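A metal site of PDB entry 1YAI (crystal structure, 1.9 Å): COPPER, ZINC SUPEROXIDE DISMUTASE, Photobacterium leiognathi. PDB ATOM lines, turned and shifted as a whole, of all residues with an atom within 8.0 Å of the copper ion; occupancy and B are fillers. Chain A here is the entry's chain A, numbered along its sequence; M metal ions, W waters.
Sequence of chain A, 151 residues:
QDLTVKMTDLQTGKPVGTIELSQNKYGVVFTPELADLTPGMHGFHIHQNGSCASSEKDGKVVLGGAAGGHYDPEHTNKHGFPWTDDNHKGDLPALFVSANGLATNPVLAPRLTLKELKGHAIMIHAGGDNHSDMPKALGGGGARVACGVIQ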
ATOM      1  N   GLY A  43      12.788   4.889 -12.442  1.00  0.00           N
ATOM      2  CA  GLY A  43      14.214   4.979 -12.295  1.00  0.00           C
ATOM      3  C   GLY A  43      14.410   5.570 -10.909  1.00  0.00           C
ATOM      4  O   GLY A  43      13.698   6.507 -10.536  1.00  0.00           O
ATOM      5  N   PHE A  44      15.379   5.047 -10.189  1.00  0.00           N
ATOM      6  CA  PHE A  44      15.655   5.399  -8.799  1.00  0.00           C
ATOM      7  C   PHE A  44      17.168   5.472  -8.632  1.00  0.00           C
ATOM      8  O   PHE A  44      17.859   4.446  -8.733  1.00  0.00           O
ATOM      9  CB  PHE A  44      15.044   4.226  -7.983  1.00  0.00           C
ATOM     10  CG  PHE A  44      15.003   4.383  -6.463  1.00  0.00           C
ATOM     11  CD1 PHE A  44      14.582   5.590  -5.907  1.00  0.00           C
ATOM     12  CD2 PHE A  44      15.388   3.350  -5.610  1.00  0.00           C
ATOM     13  CE1 PHE A  44      14.510   5.788  -4.529  1.00  0.00           C
ATOM     14  CE2 PHE A  44      15.281   3.523  -4.216  1.00  0.00           C
ATOM     15  CZ  PHE A  44      14.904   4.753  -3.673  1.00  0.00           C
ATOM     16  N   HIS A  45      17.675   6.675  -8.348  1.00  0.00           N
ATOM     17  CA  HIS A  45      19.118   6.833  -8.262  1.00  0.00           C
ATOM     18  C   HIS A  45      19.547   7.853  -7.242  1.00  0.00           C
ATOM     19  O   HIS A  45      18.769   8.744  -6.867  1.00  0.00           O
ATOM     20  CB  HIS A  45      19.694   7.374  -9.616  1.00  0.00           C
ATOM     21  CG  HIS A  45      19.036   6.874 -10.879  1.00  0.00           C
ATOM     22  ND1 HIS A  45      18.360   7.700 -11.751  1.00  0.00           N
ATOM     23  CD2 HIS A  45      18.936   5.591 -11.363  1.00  0.00           C
ATOM     24  CE1 HIS A  45      17.903   6.957 -12.745  1.00  0.00           C
ATOM     25  NE2 HIS A  45      18.219   5.668 -12.527  1.00  0.00           N
ATOM     26  N   ILE A  46      20.829   7.767  -6.892  1.00  0.00           N
ATOM     27  CA  ILE A  46      21.389   8.764  -6.016  1.00  0.00           C
ATOM     28  C   ILE A  46      22.084   9.760  -6.940  1.00  0.00           C
ATOM     29  O   ILE A  46      22.871   9.380  -7.818  1.00  0.00           O
ATOM     30  CB  ILE A  46      22.476   8.189  -5.126  1.00  0.00           C
ATOM     31  CG1 ILE A  46      21.928   7.050  -4.260  1.00  0.00           C
ATOM     32  CG2 ILE A  46      23.055   9.322  -4.278  1.00  0.00           C
ATOM     33  CD1 ILE A  46      20.968   7.536  -3.199  1.00  0.00           C
ATOM     34  N   HIS A  47      21.780  11.059  -6.778  1.00  0.00           N
ATOM     35  CA  HIS A  47      22.399  12.116  -7.593  1.00  0.00           C
ATOM     36  C   HIS A  47      23.471  12.852  -6.810  1.00  0.00           C
ATOM     37  O   HIS A  47      23.460  12.852  -5.580  1.00  0.00           O
ATOM     38  CB  HIS A  47      21.361  13.107  -8.114  1.00  0.00           C
ATOM     39  CG  HIS A  47      20.597  12.564  -9.277  1.00  0.00           C
ATOM     40  ND1 HIS A  47      20.530  13.247 -10.497  1.00  0.00           N
ATOM     41  CD2 HIS A  47      19.903  11.413  -9.400  1.00  0.00           C
ATOM     42  CE1 HIS A  47      19.804  12.507 -11.343  1.00  0.00           C
ATOM     43  NE2 HIS A  47      19.434  11.410 -10.700  1.00  0.00           N
ATOM     44  N   ALA A  67      20.042  18.851  -8.650  1.00  0.00           N
ATOM     45  CA  ALA A  67      20.717  17.715  -8.070  1.00  0.00           C
ATOM     46  C   ALA A  67      21.872  17.247  -8.926  1.00  0.00           C
ATOM     47  O   ALA A  67      22.638  16.388  -8.531  1.00  0.00           O
ATOM     48  CB  ALA A  67      19.726  16.578  -7.949  1.00  0.00           C
ATOM     49  N   GLY A  68      21.992  17.795 -10.134  1.00  0.00           N
ATOM     50  CA  GLY A  68      23.075  17.344 -10.966  1.00  0.00           C
ATOM     51  C   GLY A  68      22.824  15.931 -11.471  1.00  0.00           C
ATOM     52  O   GLY A  68      21.699  15.425 -11.442  1.00  0.00           O
ATOM     53  N   GLY A  69      23.895  15.278 -11.924  1.00  0.00           N
ATOM     54  CA  GLY A  69      23.831  13.948 -12.494  1.00  0.00           C
ATOM     55  C   GLY A  69      23.920  12.879 -11.421  1.00  0.00           C
ATOM     56  O   GLY A  69      23.765  13.184 -10.243  1.00  0.00           O
ATOM     57  N   HIS A  70      24.180  11.643 -11.845  1.00  0.00           N
ATOM     58  CA  HIS A  70      24.255  10.527 -10.925  1.00  0.00           C
ATOM     59  C   HIS A  70      25.524  10.569 -10.102  1.00  0.00           C
ATOM     60  O   HIS A  70      26.562  10.960 -10.624  1.00  0.00           O
ATOM     61  CB  HIS A  70      24.193   9.168 -11.649  1.00  0.00           C
ATOM     62  CG  HIS A  70      22.883   8.877 -12.289  1.00  0.00           C
ATOM     63  ND1 HIS A  70      22.647   7.668 -12.912  1.00  0.00           N
ATOM     64  CD2 HIS A  70      21.735   9.611 -12.357  1.00  0.00           C
ATOM     65  CE1 HIS A  70      21.397   7.699 -13.342  1.00  0.00           C
ATOM     66  NE2 HIS A  70      20.831   8.857 -13.047  1.00  0.00           N
ATOM     67  N   TYR A  71      25.405  10.144  -8.830  1.00  0.00           N
ATOM     68  CA  TYR A  71      26.497  10.049  -7.917  1.00  0.00           C
ATOM     69  C   TYR A  71      27.490   9.135  -8.585  1.00  0.00           C
ATOM     70  O   TYR A  71      27.201   7.976  -8.892  1.00  0.00           O
ATOM     71  CB  TYR A  71      25.986   9.439  -6.568  1.00  0.00           C
ATOM     72  CG  TYR A  71      27.059   9.169  -5.537  1.00  0.00           C
ATOM     73  CD1 TYR A  71      27.963  10.179  -5.169  1.00  0.00           C
ATOM     74  CD2 TYR A  71      27.160   7.927  -4.909  1.00  0.00           C
ATOM     75  CE1 TYR A  71      28.916   9.942  -4.179  1.00  0.00           C
ATOM     76  CE2 TYR A  71      28.126   7.668  -3.937  1.00  0.00           C
ATOM     77  CZ  TYR A  71      28.984   8.694  -3.580  1.00  0.00           C
ATOM     78  OH  TYR A  71      29.933   8.448  -2.639  1.00  0.00           O
ATOM     79  N   HIS A  79      26.126   4.927 -16.986  1.00  0.00           N
ATOM     80  CA  HIS A  79      25.019   4.386 -16.214  1.00  0.00           C
ATOM     81  C   HIS A  79      25.000   2.866 -16.349  1.00  0.00           C
ATOM     82  O   HIS A  79      25.299   2.343 -17.404  1.00  0.00           O
ATOM     83  CB  HIS A  79      23.729   5.006 -16.774  1.00  0.00           C
ATOM     84  CG  HIS A  79      22.526   4.580 -15.978  1.00  0.00           C
ATOM     85  ND1 HIS A  79      22.326   5.084 -14.691  1.00  0.00           N
ATOM     86  CD2 HIS A  79      21.508   3.718 -16.259  1.00  0.00           C
ATOM     87  CE1 HIS A  79      21.203   4.545 -14.201  1.00  0.00           C
ATOM     88  NE2 HIS A  79      20.674   3.709 -15.151  1.00  0.00           N
ATOM     89  N   HIS A  88      28.031   4.479 -12.553  1.00  0.00           N
ATOM     90  CA  HIS A  88      27.666   5.315 -11.417  1.00  0.00           C
ATOM     91  C   HIS A  88      27.379   4.506 -10.126  1.00  0.00           C
ATOM     92  O   HIS A  88      26.496   3.631 -10.075  1.00  0.00           O
ATOM     93  CB  HIS A  88      26.411   6.154 -11.704  1.00  0.00           C
ATOM     94  CG  HIS A  88      26.435   6.929 -12.990  1.00  0.00           C
ATOM     95  ND1 HIS A  88      25.352   6.967 -13.848  1.00  0.00           N
ATOM     96  CD2 HIS A  88      27.437   7.627 -13.556  1.00  0.00           C
ATOM     97  CE1 HIS A  88      25.672   7.701 -14.882  1.00  0.00           C
ATOM     98  NE2 HIS A  88      26.913   8.125 -14.727  1.00  0.00           N
ATOM     99  N   GLY A  90      25.791   5.646  -7.814  1.00  0.00           N
ATOM    100  CA  GLY A  90      24.454   6.024  -7.396  1.00  0.00           C
ATOM    101  C   GLY A  90      23.334   5.230  -8.093  1.00  0.00           C
ATOM    102  O   GLY A  90      22.176   5.529  -7.910  1.00  0.00           O
ATOM    103  N   ASP A  91      23.653   4.195  -8.902  1.00  0.00           N
ATOM    104  CA  ASP A  91      22.657   3.431  -9.615  1.00  0.00           C
ATOM    105  C   ASP A  91      21.963   2.396  -8.739  1.00  0.00           C
ATOM    106  O   ASP A  91      22.573   1.381  -8.451  1.00  0.00           O
ATOM    107  CB  ASP A  91      23.237   2.799 -10.924  1.00  0.00           C
ATOM    108  CG  ASP A  91      23.668   3.891 -11.909  1.00  0.00           C
ATOM    109  OD1 ASP A  91      23.189   5.014 -11.924  1.00  0.00           O
ATOM    110  OD2 ASP A  91      24.617   3.482 -12.712  1.00  0.00           O
ATOM    111  N   ALA A 121      21.304  13.586  -3.119  1.00  0.00           N
ATOM    112  CA  ALA A 121      19.871  13.484  -3.283  1.00  0.00           C
ATOM    113  C   ALA A 121      19.448  12.120  -3.828  1.00  0.00           C
ATOM    114  O   ALA A 121      20.152  11.531  -4.639  1.00  0.00           O
ATOM    115  CB  ALA A 121      19.428  14.576  -4.258  1.00  0.00           C
ATOM    116  N   ILE A 122      18.281  11.658  -3.378  1.00  0.00           N
ATOM    117  CA  ILE A 122      17.622  10.451  -3.856  1.00  0.00           C
ATOM    118  C   ILE A 122      16.591  10.928  -4.879  1.00  0.00           C
ATOM    119  O   ILE A 122      15.777  11.833  -4.650  1.00  0.00           O
ATOM    120  CB  ILE A 122      16.891   9.674  -2.757  1.00  0.00           C
ATOM    121  CG1 ILE A 122      17.842   9.343  -1.626  1.00  0.00           C
ATOM    122  CG2 ILE A 122      16.334   8.352  -3.357  1.00  0.00           C
ATOM    123  CD1 ILE A 122      17.265   8.348  -0.638  1.00  0.00           C
ATOM    124  N   MET A 123      16.611  10.328  -6.045  1.00  0.00           N
ATOM    125  CA  MET A 123      15.707  10.786  -7.092  1.00  0.00           C
ATOM    126  C   MET A 123      14.872   9.656  -7.665  1.00  0.00           C
ATOM    127  O   MET A 123      15.368   8.567  -7.887  1.00  0.00           O
ATOM    128  CB  MET A 123      16.566  11.385  -8.219  1.00  0.00           C
ATOM    129  CG  MET A 123      15.858  12.280  -9.218  1.00  0.00           C
ATOM    130  SD  MET A 123      15.435  13.888  -8.553  1.00  0.00           S
ATOM    131  CE  MET A 123      17.041  14.703  -8.464  1.00  0.00           C
ATOM    132  N   ILE A 124      13.618   9.935  -7.982  1.00  0.00           N
ATOM    133  CA  ILE A 124      12.724   9.023  -8.619  1.00  0.00           C
ATOM    134  C   ILE A 124      12.363   9.715  -9.923  1.00  0.00           C
ATOM    135  O   ILE A 124      11.998  10.899  -9.943  1.00  0.00           O
ATOM    136  CB  ILE A 124      11.452   8.828  -7.776  1.00  0.00           C
ATOM    137  CG1 ILE A 124      11.883   8.189  -6.479  1.00  0.00           C
ATOM    138  CG2 ILE A 124      10.472   7.959  -8.555  1.00  0.00           C
ATOM    139  CD1 ILE A 124      10.733   7.995  -5.501  1.00  0.00           C
ATOM    140  N   HIS A 125      12.405   8.980 -11.000  1.00  0.00           N
ATOM    141  CA  HIS A 125      12.126   9.456 -12.375  1.00  0.00           C
ATOM    142  C   HIS A 125      10.783   8.995 -12.919  1.00  0.00           C
ATOM    143  O   HIS A 125      10.154   8.063 -12.388  1.00  0.00           O
ATOM    144  CB  HIS A 125      13.217   8.988 -13.343  1.00  0.00           C
ATOM    145  CG  HIS A 125      14.579   9.526 -13.020  1.00  0.00           C
ATOM    146  ND1 HIS A 125      15.139  10.608 -13.706  1.00  0.00           N
ATOM    147  CD2 HIS A 125      15.476   9.149 -12.049  1.00  0.00           C
ATOM    148  CE1 HIS A 125      16.337  10.850 -13.167  1.00  0.00           C
ATOM    149  NE2 HIS A 125      16.561  10.011 -12.170  1.00  0.00           N
ATOM    150  N   ASP A 129      14.109   2.201 -15.745  1.00  0.00           N
ATOM    151  CA  ASP A 129      15.541   2.112 -15.762  1.00  0.00           C
ATOM    152  C   ASP A 129      15.949   0.743 -16.266  1.00  0.00           C
ATOM    153  O   ASP A 129      15.722  -0.204 -15.568  1.00  0.00           O
ATOM    154  CB  ASP A 129      16.122   2.249 -14.342  1.00  0.00           C
ATOM    155  CG  ASP A 129      17.597   2.559 -14.308  1.00  0.00           C
ATOM    156  OD1 ASP A 129      18.304   2.424 -15.265  1.00  0.00           O
ATOM    157  OD2 ASP A 129      18.020   3.092 -13.180  1.00  0.00           O
ATOM    158  N   LEU A 138      21.179   7.277 -19.432  1.00  0.00           N
ATOM    159  CA  LEU A 138      20.759   7.126 -18.063  1.00  0.00           C
ATOM    160  C   LEU A 138      19.580   6.187 -17.808  1.00  0.00           C
ATOM    161  O   LEU A 138      18.769   6.440 -16.913  1.00  0.00           O
ATOM    162  CB  LEU A 138      20.561   8.483 -17.380  1.00  0.00           C
ATOM    163  CG  LEU A 138      21.710   9.410 -17.755  1.00  0.00           C
ATOM    164  CD1 LEU A 138      21.363  10.906 -17.467  1.00  0.00           C
ATOM    165  CD2 LEU A 138      22.974   8.991 -17.001  1.00  0.00           C
ATOM    166  N   GLY A 141      15.184   7.064 -17.681  1.00  0.00           N
ATOM    167  CA  GLY A 141      14.367   7.581 -16.605  1.00  0.00           C
ATOM    168  C   GLY A 141      13.716   8.896 -16.932  1.00  0.00           C
ATOM    169  O   GLY A 141      12.632   9.149 -16.496  1.00  0.00           O
ATOM    170  N   GLY A 142      14.344   9.734 -17.750  1.00  0.00           N
ATOM    171  CA  GLY A 142      13.672  10.971 -18.119  1.00  0.00           C
ATOM    172  C   GLY A 142      13.494  11.955 -16.985  1.00  0.00           C
ATOM    173  O   GLY A 142      14.393  12.140 -16.152  1.00  0.00           O
ATOM    174  N   ALA A 143      12.370  12.650 -16.998  1.00  0.00           N
ATOM    175  CA  ALA A 143      12.090  13.684 -16.043  1.00  0.00           C
ATOM    176  C   ALA A 143      12.187  13.211 -14.598  1.00  0.00           C
ATOM    177  O   ALA A 143      11.969  12.039 -14.254  1.00  0.00           O
ATOM    178  CB  ALA A 143      10.757  14.323 -16.353  1.00  0.00           C
ATOM    179  N   ARG A 144      12.502  14.159 -13.742  1.00  0.00           N
ATOM    180  CA  ARG A 144      12.565  13.933 -12.327  1.00  0.00           C
ATOM    181  C   ARG A 144      11.228  14.287 -11.733  1.00  0.00           C
ATOM    182  O   ARG A 144      10.765  15.408 -11.895  1.00  0.00           O
ATOM    183  CB  ARG A 144      13.658  14.788 -11.746  1.00  0.00           C
ATOM    184  CG  ARG A 144      15.016  14.472 -12.399  1.00  0.00           C
ATOM    185  CD  ARG A 144      16.047  15.586 -12.282  1.00  0.00           C
ATOM    186  NE  ARG A 144      17.295  15.217 -12.989  1.00  0.00           N
ATOM    187  CZ  ARG A 144      18.560  15.548 -12.674  1.00  0.00           C
ATOM    188  NH1 ARG A 144      18.844  16.330 -11.613  1.00  0.00           N
ATOM    189  NH2 ARG A 144      19.563  15.109 -13.409  1.00  0.00           N
HETATM  190 CU    CU M   1      18.541   9.694 -11.734  1.00  0.00          CU
HETATM  191 ZN    ZN M   2      23.494   6.151 -13.352  1.00  0.00          ZN
HETATM  192  O   HOH W   1      19.076  10.853 -14.353  1.00  0.00           O
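The copper ion is bound by a ring nitrogen (ND1) of His 45 (2.0 Å), a ring nitrogen (NE2) of His 125 (2.1 Å) and a ring nitrogen (NE2) of His 47 (2.2 Å). Slightly farther from the copper ion lies a ring nitrogen (NE2) of His 70 (2.8 Å).
A ring nitrogen (ND1) of His 45 sits close to a ring nitrogen (NE2) of His 70 (3.0 Å). ND1 of His 47 is in hydrogen-bond range of O of Gly 68 (2.6 Å). The backbone carbonyl oxygen (O) of His 45 is in hydrogen-bond range of the backbone NH (N) of Met 123 (2.8 Å). N of His 125 is in hydrogen-bond range of O of Gly 43 (2.8 Å). The side-chain carboxylate of Asp 129 lies within hydrogen-bond range of a ring nitrogen (NE2) of His 45 (2.7 Å). A ring nitrogen (ND1) of His 47 lies close to the backbone carbonyl oxygen (O) of Gly 69, 3.2 Å away. N of His 47 sits at hydrogen-bond distance from O of Ala 121, 2.7 Å away. ND1 of His 125 sits at hydrogen-bond distance from O of Gly 142, at 3.0 Å.
Of the 25 residues printed, 4 come within 4 Å of the copper ion. The nearest printed residue that does not touch the copper ion is Met 123 (4.4 Å).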
